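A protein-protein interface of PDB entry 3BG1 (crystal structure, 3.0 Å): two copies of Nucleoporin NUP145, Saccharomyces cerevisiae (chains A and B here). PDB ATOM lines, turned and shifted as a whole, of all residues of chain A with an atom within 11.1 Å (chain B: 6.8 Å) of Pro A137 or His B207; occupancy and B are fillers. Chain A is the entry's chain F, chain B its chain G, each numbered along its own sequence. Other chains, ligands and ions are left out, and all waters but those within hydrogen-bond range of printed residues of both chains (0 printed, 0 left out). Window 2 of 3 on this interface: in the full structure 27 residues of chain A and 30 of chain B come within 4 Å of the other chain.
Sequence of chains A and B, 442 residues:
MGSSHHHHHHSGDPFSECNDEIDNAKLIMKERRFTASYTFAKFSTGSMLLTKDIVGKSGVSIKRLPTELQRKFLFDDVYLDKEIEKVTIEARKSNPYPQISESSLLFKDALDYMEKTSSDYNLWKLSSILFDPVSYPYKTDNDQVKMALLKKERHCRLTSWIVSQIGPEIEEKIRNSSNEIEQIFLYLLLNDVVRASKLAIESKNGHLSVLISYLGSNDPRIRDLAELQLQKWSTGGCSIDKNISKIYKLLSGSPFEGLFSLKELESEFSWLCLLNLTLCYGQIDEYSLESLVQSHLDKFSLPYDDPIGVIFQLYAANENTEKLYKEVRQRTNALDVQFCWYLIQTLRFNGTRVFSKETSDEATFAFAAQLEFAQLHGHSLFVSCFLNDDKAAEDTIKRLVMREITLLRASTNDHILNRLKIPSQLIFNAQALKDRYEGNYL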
ATOM      1  N   LYS A 108     -29.360  24.329 -46.790  1.00  0.00           N
ATOM      2  CA  LYS A 108     -30.696  23.939 -46.337  1.00  0.00           C
ATOM      3  C   LYS A 108     -31.724  24.058 -47.452  1.00  0.00           C
ATOM      4  O   LYS A 108     -32.431  23.094 -47.754  1.00  0.00           O
ATOM      5  CB  LYS A 108     -31.146  24.797 -45.141  1.00  0.00           C
ATOM      6  CG  LYS A 108     -30.216  24.720 -43.941  1.00  0.00           C
ATOM      7  CD  LYS A 108     -30.846  25.157 -42.607  1.00  0.00           C
ATOM      8  CE  LYS A 108     -29.888  24.839 -41.432  1.00  0.00           C
ATOM      9  NZ  LYS A 108     -30.414  25.166 -40.073  1.00  0.00           N
ATOM     10  N   PRO A 133     -25.429  28.512 -40.697  1.00  0.00           N
ATOM     11  CA  PRO A 133     -25.458  29.177 -39.396  1.00  0.00           C
ATOM     12  C   PRO A 133     -26.404  28.559 -38.372  1.00  0.00           C
ATOM     13  O   PRO A 133     -27.495  28.064 -38.691  1.00  0.00           O
ATOM     14  CB  PRO A 133     -25.844  30.604 -39.747  1.00  0.00           C
ATOM     15  CG  PRO A 133     -26.643  30.432 -41.011  1.00  0.00           C
ATOM     16  CD  PRO A 133     -25.828  29.431 -41.769  1.00  0.00           C
ATOM     17  N   VAL A 134     -25.951  28.596 -37.127  1.00  0.00           N
ATOM     18  CA  VAL A 134     -26.690  28.062 -36.000  1.00  0.00           C
ATOM     19  C   VAL A 134     -27.312  29.269 -35.337  1.00  0.00           C
ATOM     20  O   VAL A 134     -26.815  30.376 -35.517  1.00  0.00           O
ATOM     21  CB  VAL A 134     -25.733  27.386 -35.014  1.00  0.00           C
ATOM     22  CG1 VAL A 134     -26.519  26.678 -33.920  1.00  0.00           C
ATOM     23  CG2 VAL A 134     -24.816  26.423 -35.767  1.00  0.00           C
ATOM     24  N   SER A 135     -28.387  29.077 -34.578  1.00  0.00           N
ATOM     25  CA  SER A 135     -29.024  30.213 -33.918  1.00  0.00           C
ATOM     26  C   SER A 135     -30.002  29.957 -32.774  1.00  0.00           C
ATOM     27  O   SER A 135     -30.870  29.084 -32.838  1.00  0.00           O
ATOM     28  CB  SER A 135     -29.711  31.106 -34.962  1.00  0.00           C
ATOM     29  OG  SER A 135     -30.468  30.353 -35.891  1.00  0.00           O
ATOM     30  N   TYR A 136     -29.833  30.754 -31.724  1.00  0.00           N
ATOM     31  CA  TYR A 136     -30.668  30.733 -30.528  1.00  0.00           C
ATOM     32  C   TYR A 136     -32.040  31.184 -30.995  1.00  0.00           C
ATOM     33  O   TYR A 136     -32.170  31.878 -32.009  1.00  0.00           O
ATOM     34  CB  TYR A 136     -30.166  31.788 -29.552  1.00  0.00           C
ATOM     35  CG  TYR A 136     -30.207  33.177 -30.195  1.00  0.00           C
ATOM     36  CD1 TYR A 136     -31.382  33.945 -30.198  1.00  0.00           C
ATOM     37  CD2 TYR A 136     -29.106  33.675 -30.907  1.00  0.00           C
ATOM     38  CE1 TYR A 136     -31.461  35.170 -30.906  1.00  0.00           C
ATOM     39  CE2 TYR A 136     -29.176  34.901 -31.618  1.00  0.00           C
ATOM     40  CZ  TYR A 136     -30.354  35.638 -31.614  1.00  0.00           C
ATOM     41  OH  TYR A 136     -30.417  36.822 -32.325  1.00  0.00           O
ATOM     42  N   PRO A 137     -33.088  30.781 -30.282  1.00  0.00           N
ATOM     43  CA  PRO A 137     -34.392  31.251 -30.752  1.00  0.00           C
ATOM     44  C   PRO A 137     -35.002  32.215 -29.733  1.00  0.00           C
ATOM     45  O   PRO A 137     -36.204  32.473 -29.750  1.00  0.00           O
ATOM     46  CB  PRO A 137     -35.188  29.963 -30.912  1.00  0.00           C
ATOM     47  CG  PRO A 137     -34.711  29.166 -29.771  1.00  0.00           C
ATOM     48  CD  PRO A 137     -33.206  29.467 -29.634  1.00  0.00           C
ATOM     49  N   TYR A 138     -34.160  32.738 -28.842  1.00  0.00           N
ATOM     50  CA  TYR A 138     -34.596  33.693 -27.820  1.00  0.00           C
ATOM     51  C   TYR A 138     -33.419  34.634 -27.528  1.00  0.00           C
ATOM     52  O   TYR A 138     -32.271  34.184 -27.479  1.00  0.00           O
ATOM     53  CB  TYR A 138     -35.033  32.953 -26.550  1.00  0.00           C
ATOM     54  CG  TYR A 138     -36.004  31.803 -26.791  1.00  0.00           C
ATOM     55  CD1 TYR A 138     -35.548  30.478 -26.863  1.00  0.00           C
ATOM     56  CD2 TYR A 138     -37.372  32.035 -26.939  1.00  0.00           C
ATOM     57  CE1 TYR A 138     -36.438  29.412 -27.072  1.00  0.00           C
ATOM     58  CE2 TYR A 138     -38.267  30.978 -27.151  1.00  0.00           C
ATOM     59  CZ  TYR A 138     -37.795  29.670 -27.216  1.00  0.00           C
ATOM     60  OH  TYR A 138     -38.677  28.628 -27.419  1.00  0.00           O
ATOM     61  N   LYS A 139     -33.697  35.923 -27.313  1.00  0.00           N
ATOM     62  CA  LYS A 139     -32.618  36.898 -27.106  1.00  0.00           C
ATOM     63  C   LYS A 139     -31.888  37.062 -25.761  1.00  0.00           C
ATOM     64  O   LYS A 139     -32.070  38.053 -25.053  1.00  0.00           O
ATOM     65  CB  LYS A 139     -33.051  38.293 -27.633  1.00  0.00           C
ATOM     66  CG  LYS A 139     -34.103  39.101 -26.837  1.00  0.00           C
ATOM     67  CD  LYS A 139     -34.314  40.491 -27.506  1.00  0.00           C
ATOM     68  CE  LYS A 139     -35.068  41.487 -26.623  1.00  0.00           C
ATOM     69  NZ  LYS A 139     -35.117  42.847 -27.244  1.00  0.00           N
ATOM     70  N   THR A 140     -31.043  36.084 -25.436  1.00  0.00           N
ATOM     71  CA  THR A 140     -30.214  36.120 -24.231  1.00  0.00           C
ATOM     72  C   THR A 140     -28.832  36.456 -24.766  1.00  0.00           C
ATOM     73  O   THR A 140     -28.386  35.864 -25.753  1.00  0.00           O
ATOM     74  CB  THR A 140     -30.146  34.766 -23.515  1.00  0.00           C
ATOM     75  OG1 THR A 140     -31.325  34.585 -22.722  1.00  0.00           O
ATOM     76  CG2 THR A 140     -28.906  34.700 -22.619  1.00  0.00           C
ATOM     77  N   ASP A 141     -28.130  37.368 -24.108  1.00  0.00           N
ATOM     78  CA  ASP A 141     -26.854  37.782 -24.655  1.00  0.00           C
ATOM     79  C   ASP A 141     -25.559  37.616 -23.900  1.00  0.00           C
ATOM     80  O   ASP A 141     -24.648  38.422 -24.064  1.00  0.00           O
ATOM     81  CB  ASP A 141     -26.973  39.234 -25.096  1.00  0.00           C
ATOM     82  CG  ASP A 141     -27.251  40.164 -23.939  1.00  0.00           C
ATOM     83  OD1 ASP A 141     -27.640  39.666 -22.858  1.00  0.00           O
ATOM     84  OD2 ASP A 141     -27.083  41.389 -24.119  1.00  0.00           O
ATOM     85  N   VAL A 145     -22.060  32.778 -23.282  1.00  0.00           N
ATOM     86  CA  VAL A 145     -23.054  31.705 -23.318  1.00  0.00           C
ATOM     87  C   VAL A 145     -23.538  31.424 -24.739  1.00  0.00           C
ATOM     88  O   VAL A 145     -23.344  30.329 -25.263  1.00  0.00           O
ATOM     89  CB  VAL A 145     -24.256  32.057 -22.402  1.00  0.00           C
ATOM     90  CG1 VAL A 145     -25.529  31.424 -22.921  1.00  0.00           C
ATOM     91  CG2 VAL A 145     -23.969  31.579 -20.975  1.00  0.00           C
ATOM     92  N   LYS A 146     -24.176  32.415 -25.353  1.00  0.00           N
ATOM     93  CA  LYS A 146     -24.663  32.272 -26.714  1.00  0.00           C
ATOM     94  C   LYS A 146     -23.572  31.626 -27.577  1.00  0.00           C
ATOM     95  O   LYS A 146     -23.833  30.667 -28.297  1.00  0.00           O
ATOM     96  CB  LYS A 146     -25.058  33.644 -27.274  1.00  0.00           C
ATOM     97  CG  LYS A 146     -25.510  33.638 -28.730  1.00  0.00           C
ATOM     98  CD  LYS A 146     -26.050  35.004 -29.174  1.00  0.00           C
ATOM     99  CE  LYS A 146     -27.323  35.392 -28.418  1.00  0.00           C
ATOM    100  NZ  LYS A 146     -27.912  36.670 -28.918  1.00  0.00           N
ATOM    101  N   ALA A 148     -21.273  29.731 -26.678  1.00  0.00           N
ATOM    102  CA  ALA A 148     -21.034  28.358 -26.247  1.00  0.00           C
ATOM    103  C   ALA A 148     -22.176  27.438 -26.679  1.00  0.00           C
ATOM    104  O   ALA A 148     -21.961  26.253 -26.922  1.00  0.00           O
ATOM    105  CB  ALA A 148     -20.864  28.307 -24.742  1.00  0.00           C
ATOM    106  N   LEU A 149     -23.388  27.986 -26.762  1.00  0.00           N
ATOM    107  CA  LEU A 149     -24.551  27.206 -27.178  1.00  0.00           C
ATOM    108  C   LEU A 149     -24.386  26.800 -28.613  1.00  0.00           C
ATOM    109  O   LEU A 149     -24.277  25.621 -28.918  1.00  0.00           O
ATOM    110  CB  LEU A 149     -25.836  28.013 -27.051  1.00  0.00           C
ATOM    111  CG  LEU A 149     -26.323  28.172 -25.615  1.00  0.00           C
ATOM    112  CD1 LEU A 149     -27.733  28.775 -25.609  1.00  0.00           C
ATOM    113  CD2 LEU A 149     -26.292  26.802 -24.920  1.00  0.00           C
ATOM    114  N   LEU A 150     -24.385  27.792 -29.496  1.00  0.00           N
ATOM    115  CA  LEU A 150     -24.204  27.545 -30.916  1.00  0.00           C
ATOM    116  C   LEU A 150     -23.031  26.577 -31.073  1.00  0.00           C
ATOM    117  O   LEU A 150     -23.071  25.661 -31.895  1.00  0.00           O
ATOM    118  CB  LEU A 150     -23.889  28.854 -31.634  1.00  0.00           C
ATOM    119  CG  LEU A 150     -24.712  30.080 -31.234  1.00  0.00           C
ATOM    120  CD1 LEU A 150     -24.309  31.259 -32.114  1.00  0.00           C
ATOM    121  CD2 LEU A 150     -26.198  29.792 -31.372  1.00  0.00           C
ATOM    122  N   LYS A 151     -21.985  26.792 -30.280  1.00  0.00           N
ATOM    123  CA  LYS A 151     -20.813  25.924 -30.309  1.00  0.00           C
ATOM    124  C   LYS A 151     -21.297  24.480 -30.202  1.00  0.00           C
ATOM    125  O   LYS A 151     -20.917  23.628 -31.008  1.00  0.00           O
ATOM    126  CB  LYS A 151     -19.870  26.273 -29.136  1.00  0.00           C
ATOM    127  CG  LYS A 151     -19.345  25.089 -28.290  1.00  0.00           C
ATOM    128  CD  LYS A 151     -18.177  24.327 -28.934  1.00  0.00           C
ATOM    129  CE  LYS A 151     -17.678  23.207 -28.010  1.00  0.00           C
ATOM    130  NZ  LYS A 151     -16.504  22.456 -28.549  1.00  0.00           N
ATOM    131  N   LYS A 152     -22.158  24.225 -29.213  1.00  0.00           N
ATOM    132  CA  LYS A 152     -22.705  22.891 -28.974  1.00  0.00           C
ATOM    133  C   LYS A 152     -23.831  22.500 -29.939  1.00  0.00           C
ATOM    134  O   LYS A 152     -23.815  21.395 -30.482  1.00  0.00           O
ATOM    135  CB  LYS A 152     -23.201  22.771 -27.524  1.00  0.00           C
ATOM    136  CG  LYS A 152     -23.590  21.355 -27.116  1.00  0.00           C
ATOM    137  CD  LYS A 152     -22.812  20.882 -25.894  1.00  0.00           C
ATOM    138  CE  LYS A 152     -22.645  19.358 -25.898  1.00  0.00           C
ATOM    139  NZ  LYS A 152     -21.823  18.843 -24.753  1.00  0.00           N
ATOM    140  N   GLU A 153     -24.808  23.385 -30.154  1.00  0.00           N
ATOM    141  CA  GLU A 153     -25.897  23.054 -31.063  1.00  0.00           C
ATOM    142  C   GLU A 153     -25.298  22.432 -32.295  1.00  0.00           C
ATOM    143  O   GLU A 153     -25.734  21.383 -32.753  1.00  0.00           O
ATOM    144  CB  GLU A 153     -26.708  24.277 -31.475  1.00  0.00           C
ATOM    145  CG  GLU A 153     -27.740  23.911 -32.525  1.00  0.00           C
ATOM    146  CD  GLU A 153     -28.897  24.893 -32.623  1.00  0.00           C
ATOM    147  OE1 GLU A 153     -29.519  25.196 -31.580  1.00  0.00           O
ATOM    148  OE2 GLU A 153     -29.204  25.351 -33.746  1.00  0.00           O
ATOM    149  N   ARG A 154     -24.275  23.068 -32.832  1.00  0.00           N
ATOM    150  CA  ARG A 154     -23.653  22.514 -34.006  1.00  0.00           C
ATOM    151  C   ARG A 154     -23.071  21.151 -33.689  1.00  0.00           C
ATOM    152  O   ARG A 154     -23.049  20.271 -34.541  1.00  0.00           O
ATOM    153  CB  ARG A 154     -22.552  23.426 -34.532  1.00  0.00           C
ATOM    154  CG  ARG A 154     -21.774  22.768 -35.641  1.00  0.00           C
ATOM    155  CD  ARG A 154     -21.166  23.771 -36.551  1.00  0.00           C
ATOM    156  NE  ARG A 154     -22.167  24.737 -36.963  1.00  0.00           N
ATOM    157  CZ  ARG A 154     -21.936  25.685 -37.856  1.00  0.00           C
ATOM    158  NH1 ARG A 154     -20.735  25.766 -38.419  1.00  0.00           N
ATOM    159  NH2 ARG A 154     -22.888  26.555 -38.169  1.00  0.00           N
ATOM    160  N   HIS A 155     -22.606  20.959 -32.464  1.00  0.00           N
ATOM    161  CA  HIS A 155     -22.011  19.681 -32.108  1.00  0.00           C
ATOM    162  C   HIS A 155     -22.998  18.529 -32.201  1.00  0.00           C
ATOM    163  O   HIS A 155     -22.804  17.596 -32.986  1.00  0.00           O
ATOM    164  CB  HIS A 155     -21.417  19.742 -30.703  1.00  0.00           C
ATOM    165  CG  HIS A 155     -20.603  18.540 -30.346  1.00  0.00           C
ATOM    166  ND1 HIS A 155     -21.166  17.305 -30.110  1.00  0.00           N
ATOM    167  CD2 HIS A 155     -19.265  18.377 -30.213  1.00  0.00           C
ATOM    168  CE1 HIS A 155     -20.211  16.433 -29.846  1.00  0.00           C
ATOM    169  NE2 HIS A 155     -19.047  17.059 -29.901  1.00  0.00           N
ATOM    170  N   CYS A 156     -24.057  18.593 -31.405  1.00  0.00           N
ATOM    171  CA  CYS A 156     -25.060  17.542 -31.422  1.00  0.00           C
ATOM    172  C   CYS A 156     -25.503  17.344 -32.851  1.00  0.00           C
ATOM    173  O   CYS A 156     -25.337  16.267 -33.425  1.00  0.00           O
ATOM    174  CB  CYS A 156     -26.260  17.947 -30.594  1.00  0.00           C
ATOM    175  SG  CYS A 156     -25.797  18.794 -29.101  1.00  0.00           S
ATOM    176  N   ARG A 157     -26.066  18.401 -33.423  1.00  0.00           N
ATOM    177  CA  ARG A 157     -26.547  18.356 -34.794  1.00  0.00           C
ATOM    178  C   ARG A 157     -25.730  17.424 -35.664  1.00  0.00           C
ATOM    179  O   ARG A 157     -26.283  16.612 -36.411  1.00  0.00           O
ATOM    180  CB  ARG A 157     -26.540  19.749 -35.398  1.00  0.00           C
ATOM    181  CG  ARG A 157     -27.857  20.445 -35.256  1.00  0.00           C
ATOM    182  CD  ARG A 157     -28.793  20.107 -36.412  1.00  0.00           C
ATOM    183  NE  ARG A 157     -30.155  20.601 -36.184  1.00  0.00           N
ATOM    184  CZ  ARG A 157     -30.459  21.778 -35.631  1.00  0.00           C
ATOM    185  NH1 ARG A 157     -29.499  22.605 -35.237  1.00  0.00           N
ATOM    186  NH2 ARG A 157     -31.731  22.134 -35.462  1.00  0.00           N
ATOM    187  N   SER A 160     -25.491  13.743 -33.975  1.00  0.00           N
ATOM    188  CA  SER A 160     -26.840  13.225 -34.133  1.00  0.00           C
ATOM    189  C   SER A 160     -27.084  12.709 -35.544  1.00  0.00           C
ATOM    190  O   SER A 160     -27.875  11.791 -35.750  1.00  0.00           O
ATOM    191  CB  SER A 160     -27.862  14.301 -33.781  1.00  0.00           C
ATOM    192  OG  SER A 160     -27.825  14.576 -32.392  1.00  0.00           O
ATOM    193  N   ALA B 200     -36.300  15.864 -30.608  1.00  0.00           N
ATOM    194  CA  ALA B 200     -36.121  17.310 -30.677  1.00  0.00           C
ATOM    195  C   ALA B 200     -35.602  17.792 -32.030  1.00  0.00           C
ATOM    196  O   ALA B 200     -36.136  18.735 -32.618  1.00  0.00           O
ATOM    197  CB  ALA B 200     -35.185  17.765 -29.565  1.00  0.00           C
ATOM    198  N   LYS B 204     -37.685  19.773 -35.802  1.00  0.00           N
ATOM    199  CA  LYS B 204     -37.271  21.137 -36.114  1.00  0.00           C
ATOM    200  C   LYS B 204     -37.417  21.975 -34.836  1.00  0.00           C
ATOM    201  O   LYS B 204     -37.933  23.100 -34.854  1.00  0.00           O
ATOM    202  CB  LYS B 204     -38.137  21.718 -37.245  1.00  0.00           C
ATOM    203  CG  LYS B 204     -37.551  22.940 -37.972  1.00  0.00           C
ATOM    204  CD  LYS B 204     -36.646  22.551 -39.148  1.00  0.00           C
ATOM    205  CE  LYS B 204     -36.164  23.784 -39.916  1.00  0.00           C
ATOM    206  NZ  LYS B 204     -35.335  23.438 -41.106  1.00  0.00           N
ATOM    207  N   ASN B 205     -36.966  21.392 -33.724  1.00  0.00           N
ATOM    208  CA  ASN B 205     -36.993  22.030 -32.410  1.00  0.00           C
ATOM    209  C   ASN B 205     -35.642  21.755 -31.767  1.00  0.00           C
ATOM    210  O   ASN B 205     -35.545  21.363 -30.605  1.00  0.00           O
ATOM    211  CB  ASN B 205     -38.113  21.435 -31.563  1.00  0.00           C
ATOM    212  CG  ASN B 205     -39.472  21.987 -31.934  1.00  0.00           C
ATOM    213  OD1 ASN B 205     -39.702  23.196 -31.846  1.00  0.00           O
ATOM    214  ND2 ASN B 205     -40.379  21.111 -32.352  1.00  0.00           N
ATOM    215  N   GLY B 206     -34.602  21.984 -32.557  1.00  0.00           N
ATOM    216  CA  GLY B 206     -33.238  21.732 -32.137  1.00  0.00           C
ATOM    217  C   GLY B 206     -32.656  22.370 -30.894  1.00  0.00           C
ATOM    218  O   GLY B 206     -32.042  21.663 -30.097  1.00  0.00           O
ATOM    219  N   HIS B 207     -32.819  23.681 -30.722  1.00  0.00           N
ATOM    220  CA  HIS B 207     -32.248  24.354 -29.557  1.00  0.00           C
ATOM    221  C   HIS B 207     -32.393  23.505 -28.298  1.00  0.00           C
ATOM    222  O   HIS B 207     -31.517  23.521 -27.429  1.00  0.00           O
ATOM    223  CB  HIS B 207     -32.896  25.720 -29.359  1.00  0.00           C
ATOM    224  CG  HIS B 207     -34.376  25.661 -29.183  1.00  0.00           C
ATOM    225  ND1 HIS B 207     -35.192  24.933 -30.021  1.00  0.00           N
ATOM    226  CD2 HIS B 207     -35.191  26.253 -28.279  1.00  0.00           C
ATOM    227  CE1 HIS B 207     -36.449  25.082 -29.641  1.00  0.00           C
ATOM    228  NE2 HIS B 207     -36.477  25.878 -28.586  1.00  0.00           N
ATOM    229  N   LEU B 208     -33.489  22.751 -28.211  1.00  0.00           N
ATOM    230  CA  LEU B 208     -33.734  21.875 -27.064  1.00  0.00           C
ATOM    231  C   LEU B 208     -32.703  20.757 -26.994  1.00  0.00           C
ATOM    232  O   LEU B 208     -32.148  20.467 -25.937  1.00  0.00           O
ATOM    233  CB  LEU B 208     -35.120  21.247 -27.150  1.00  0.00           C
ATOM    234  CG  LEU B 208     -36.329  22.182 -27.184  1.00  0.00           C
ATOM    235  CD1 LEU B 208     -37.580  21.339 -26.995  1.00  0.00           C
ATOM    236  CD2 LEU B 208     -36.252  23.239 -26.084  1.00  0.00           C
ATOM    237  N   SER B 209     -32.456  20.120 -28.126  1.00  0.00           N
ATOM    238  CA  SER B 209     -31.491  19.041 -28.158  1.00  0.00           C
ATOM    239  C   SER B 209     -30.192  19.517 -27.522  1.00  0.00           C
ATOM    240  O   SER B 209     -29.397  18.713 -27.029  1.00  0.00           O
ATOM    241  CB  SER B 209     -31.244  18.600 -29.600  1.00  0.00           C
ATOM    242  OG  SER B 209     -30.632  17.321 -29.632  1.00  0.00           O
ATOM    243  N   VAL B 210     -29.984  20.830 -27.524  1.00  0.00           N
ATOM    244  CA  VAL B 210     -28.780  21.396 -26.940  1.00  0.00           C
ATOM    245  C   VAL B 210     -28.888  21.398 -25.438  1.00  0.00           C
ATOM    246  O   VAL B 210     -28.031  20.852 -24.746  1.00  0.00           O
ATOM    247  CB  VAL B 210     -28.549  22.837 -27.380  1.00  0.00           C
ATOM    248  CG1 VAL B 210     -27.387  23.420 -26.598  1.00  0.00           C
ATOM    249  CG2 VAL B 210     -28.252  22.887 -28.862  1.00  0.00           C
ATOM    250  N   LEU B 211     -29.943  22.025 -24.934  1.00  0.00           N
ATOM    251  CA  LEU B 211     -30.156  22.093 -23.493  1.00  0.00           C
ATOM    252  C   LEU B 211     -30.170  20.673 -22.963  1.00  0.00           C
ATOM    253  O   LEU B 211     -29.421  20.345 -22.045  1.00  0.00           O
ATOM    254  CB  LEU B 211     -31.478  22.788 -23.185  1.00  0.00           C
ATOM    255  CG  LEU B 211     -31.838  23.868 -24.214  1.00  0.00           C
ATOM    256  CD1 LEU B 211     -33.006  24.696 -23.714  1.00  0.00           C
ATOM    257  CD2 LEU B 211     -30.637  24.761 -24.476  1.00  0.00           C
ATOM    258  N   ILE B 212     -31.019  19.835 -23.557  1.00  0.00           N
ATOM    259  CA  ILE B 212     -31.120  18.430 -23.179  1.00  0.00           C
ATOM    260  C   ILE B 212     -29.719  17.854 -23.016  1.00  0.00           C
ATOM    261  O   ILE B 212     -29.488  16.992 -22.174  1.00  0.00           O
ATOM    262  CB  ILE B 212     -31.865  17.626 -24.258  1.00  0.00           C
ATOM    263  CG1 ILE B 212     -33.363  17.843 -24.105  1.00  0.00           C
ATOM    264  CG2 ILE B 212     -31.517  16.155 -24.164  1.00  0.00           C
ATOM    265  CD1 ILE B 212     -34.186  17.050 -25.077  1.00  0.00           C
ATOM    266  N   GLN B 229     -34.386  33.281 -18.053  1.00  0.00           N
ATOM    267  CA  GLN B 229     -35.312  33.360 -19.166  1.00  0.00           C
ATOM    268  C   GLN B 229     -36.714  33.223 -18.618  1.00  0.00           C
ATOM    269  O   GLN B 229     -37.555  34.091 -18.841  1.00  0.00           O
ATOM    270  CB  GLN B 229     -35.038  32.271 -20.198  1.00  0.00           C
ATOM    271  CG  GLN B 229     -34.172  32.769 -21.342  1.00  0.00           C
ATOM    272  CD  GLN B 229     -34.682  32.324 -22.693  1.00  0.00           C
ATOM    273  OE1 GLN B 229     -35.888  32.359 -22.955  1.00  0.00           O
ATOM    274  NE2 GLN B 229     -33.766  31.914 -23.568  1.00  0.00           N
ATOM    275  N   ILE B 244     -42.278  23.317 -23.776  1.00  0.00           N
ATOM    276  CA  ILE B 244     -40.965  23.938 -23.869  1.00  0.00           C
ATOM    277  C   ILE B 244     -40.656  24.521 -22.508  1.00  0.00           C
ATOM    278  O   ILE B 244     -39.513  24.490 -22.061  1.00  0.00           O
ATOM    279  CB  ILE B 244     -40.901  25.058 -24.915  1.00  0.00           C
ATOM    280  CG1 ILE B 244     -41.377  24.531 -26.271  1.00  0.00           C
ATOM    281  CG2 ILE B 244     -39.467  25.543 -25.044  1.00  0.00           C
ATOM    282  CD1 ILE B 244     -41.427  25.583 -27.382  1.00  0.00           C
ATOM    283  N   TYR B 248     -37.438  23.668 -19.758  1.00  0.00           N
ATOM    284  CA  TYR B 248     -36.463  24.600 -19.217  1.00  0.00           C
ATOM    285  C   TYR B 248     -36.499  24.454 -17.701  1.00  0.00           C
ATOM    286  O   TYR B 248     -35.467  24.533 -17.030  1.00  0.00           O
ATOM    287  CB  TYR B 248     -36.792  26.037 -19.617  1.00  0.00           C
ATOM    288  CG  TYR B 248     -36.209  26.426 -20.953  1.00  0.00           C
ATOM    289  CD1 TYR B 248     -36.968  26.371 -22.120  1.00  0.00           C
ATOM    290  CD2 TYR B 248     -34.879  26.812 -21.056  1.00  0.00           C
ATOM    291  CE1 TYR B 248     -36.412  26.695 -23.365  1.00  0.00           C
ATOM    292  CE2 TYR B 248     -34.312  27.135 -22.291  1.00  0.00           C
ATOM    293  CZ  TYR B 248     -35.082  27.073 -23.443  1.00  0.00           C
ATOM    294  OH  TYR B 248     -34.512  27.386 -24.664  1.00  0.00           O
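Of the 13 printed residues of chain B, 6 touch a printed residue of chain A. Printed residues of chain B that touch a printed residue of chain A: Gly B206, His B207, Val B210, Gln B229, Ile B244 and Tyr B248. Hydrophobic or aromatic side chains of chain A that line the printed part of chain B: Pro A137, Tyr A138 and Leu A149. Among the printed residues, 10 pairs touch across the chains. Among the printed residues, no Asp or Glu carboxylate lies within 4 Å of a Lys or Arg side-chain nitrogen of the other chain.
No position is printed for both chains. Of the 10 pairs that touch across the chains among the printed residues, none has its exchanged pair printed and touching as well.
The side-chain carboxylate (OE2) of Glu A153 lies within salt-bridge range of the guanidinium group (NH1) of Arg A157 (3.1 Å). O of Thr A140 sits close to NZ of Lys A146 (3.3 Å).
Pro A137 touches just one residue of chain B: His B207. Printed residues of chain B within 4 Å of Tyr A138: His B207, Gln B229, Ile B244 and Tyr B248. Val A145 touches none of the printed residues of chain B. Printed residues of chain B within 4 Å of Leu A149: Val B210. No residue of chain A comes within 4 Å of Asn B205. His B207 touches just these residues of chain A: Pro A137 (3.3 Å), Tyr A138 (3.6 Å) and Glu A153 (3.5 Å). No residue of chain A comes within 4 Å of Ser B209. Val B210 touches just these residues of chain A: Leu A149 and Glu A153. No residue of chain A comes within 4 Å of Leu B211. Ile B212 touches none of the printed residues of chain A. The nearest printed residue of chain B that does not touch Arg A157 is His B207 (5.1 Å).
Among the printed residues, merely in contact across the chains: Pro A137 with His B207 (3.3 Å), Tyr A138 with His B207 (3.6 Å), Tyr A138 with Gln B229 (3.4 Å), Tyr A138 with Ile B244 (3.97 Å), Tyr A138 with Tyr B248 (3.7 Å), Thr A140 with Gln B229 (3.6 Å), Leu A149 with Val B210 (3.9 Å), Glu A153 with His B207 (3.5 Å), Glu A153 with Val B210 (3.2 Å) and Arg A157 with Gly B206 (3.7 Å).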
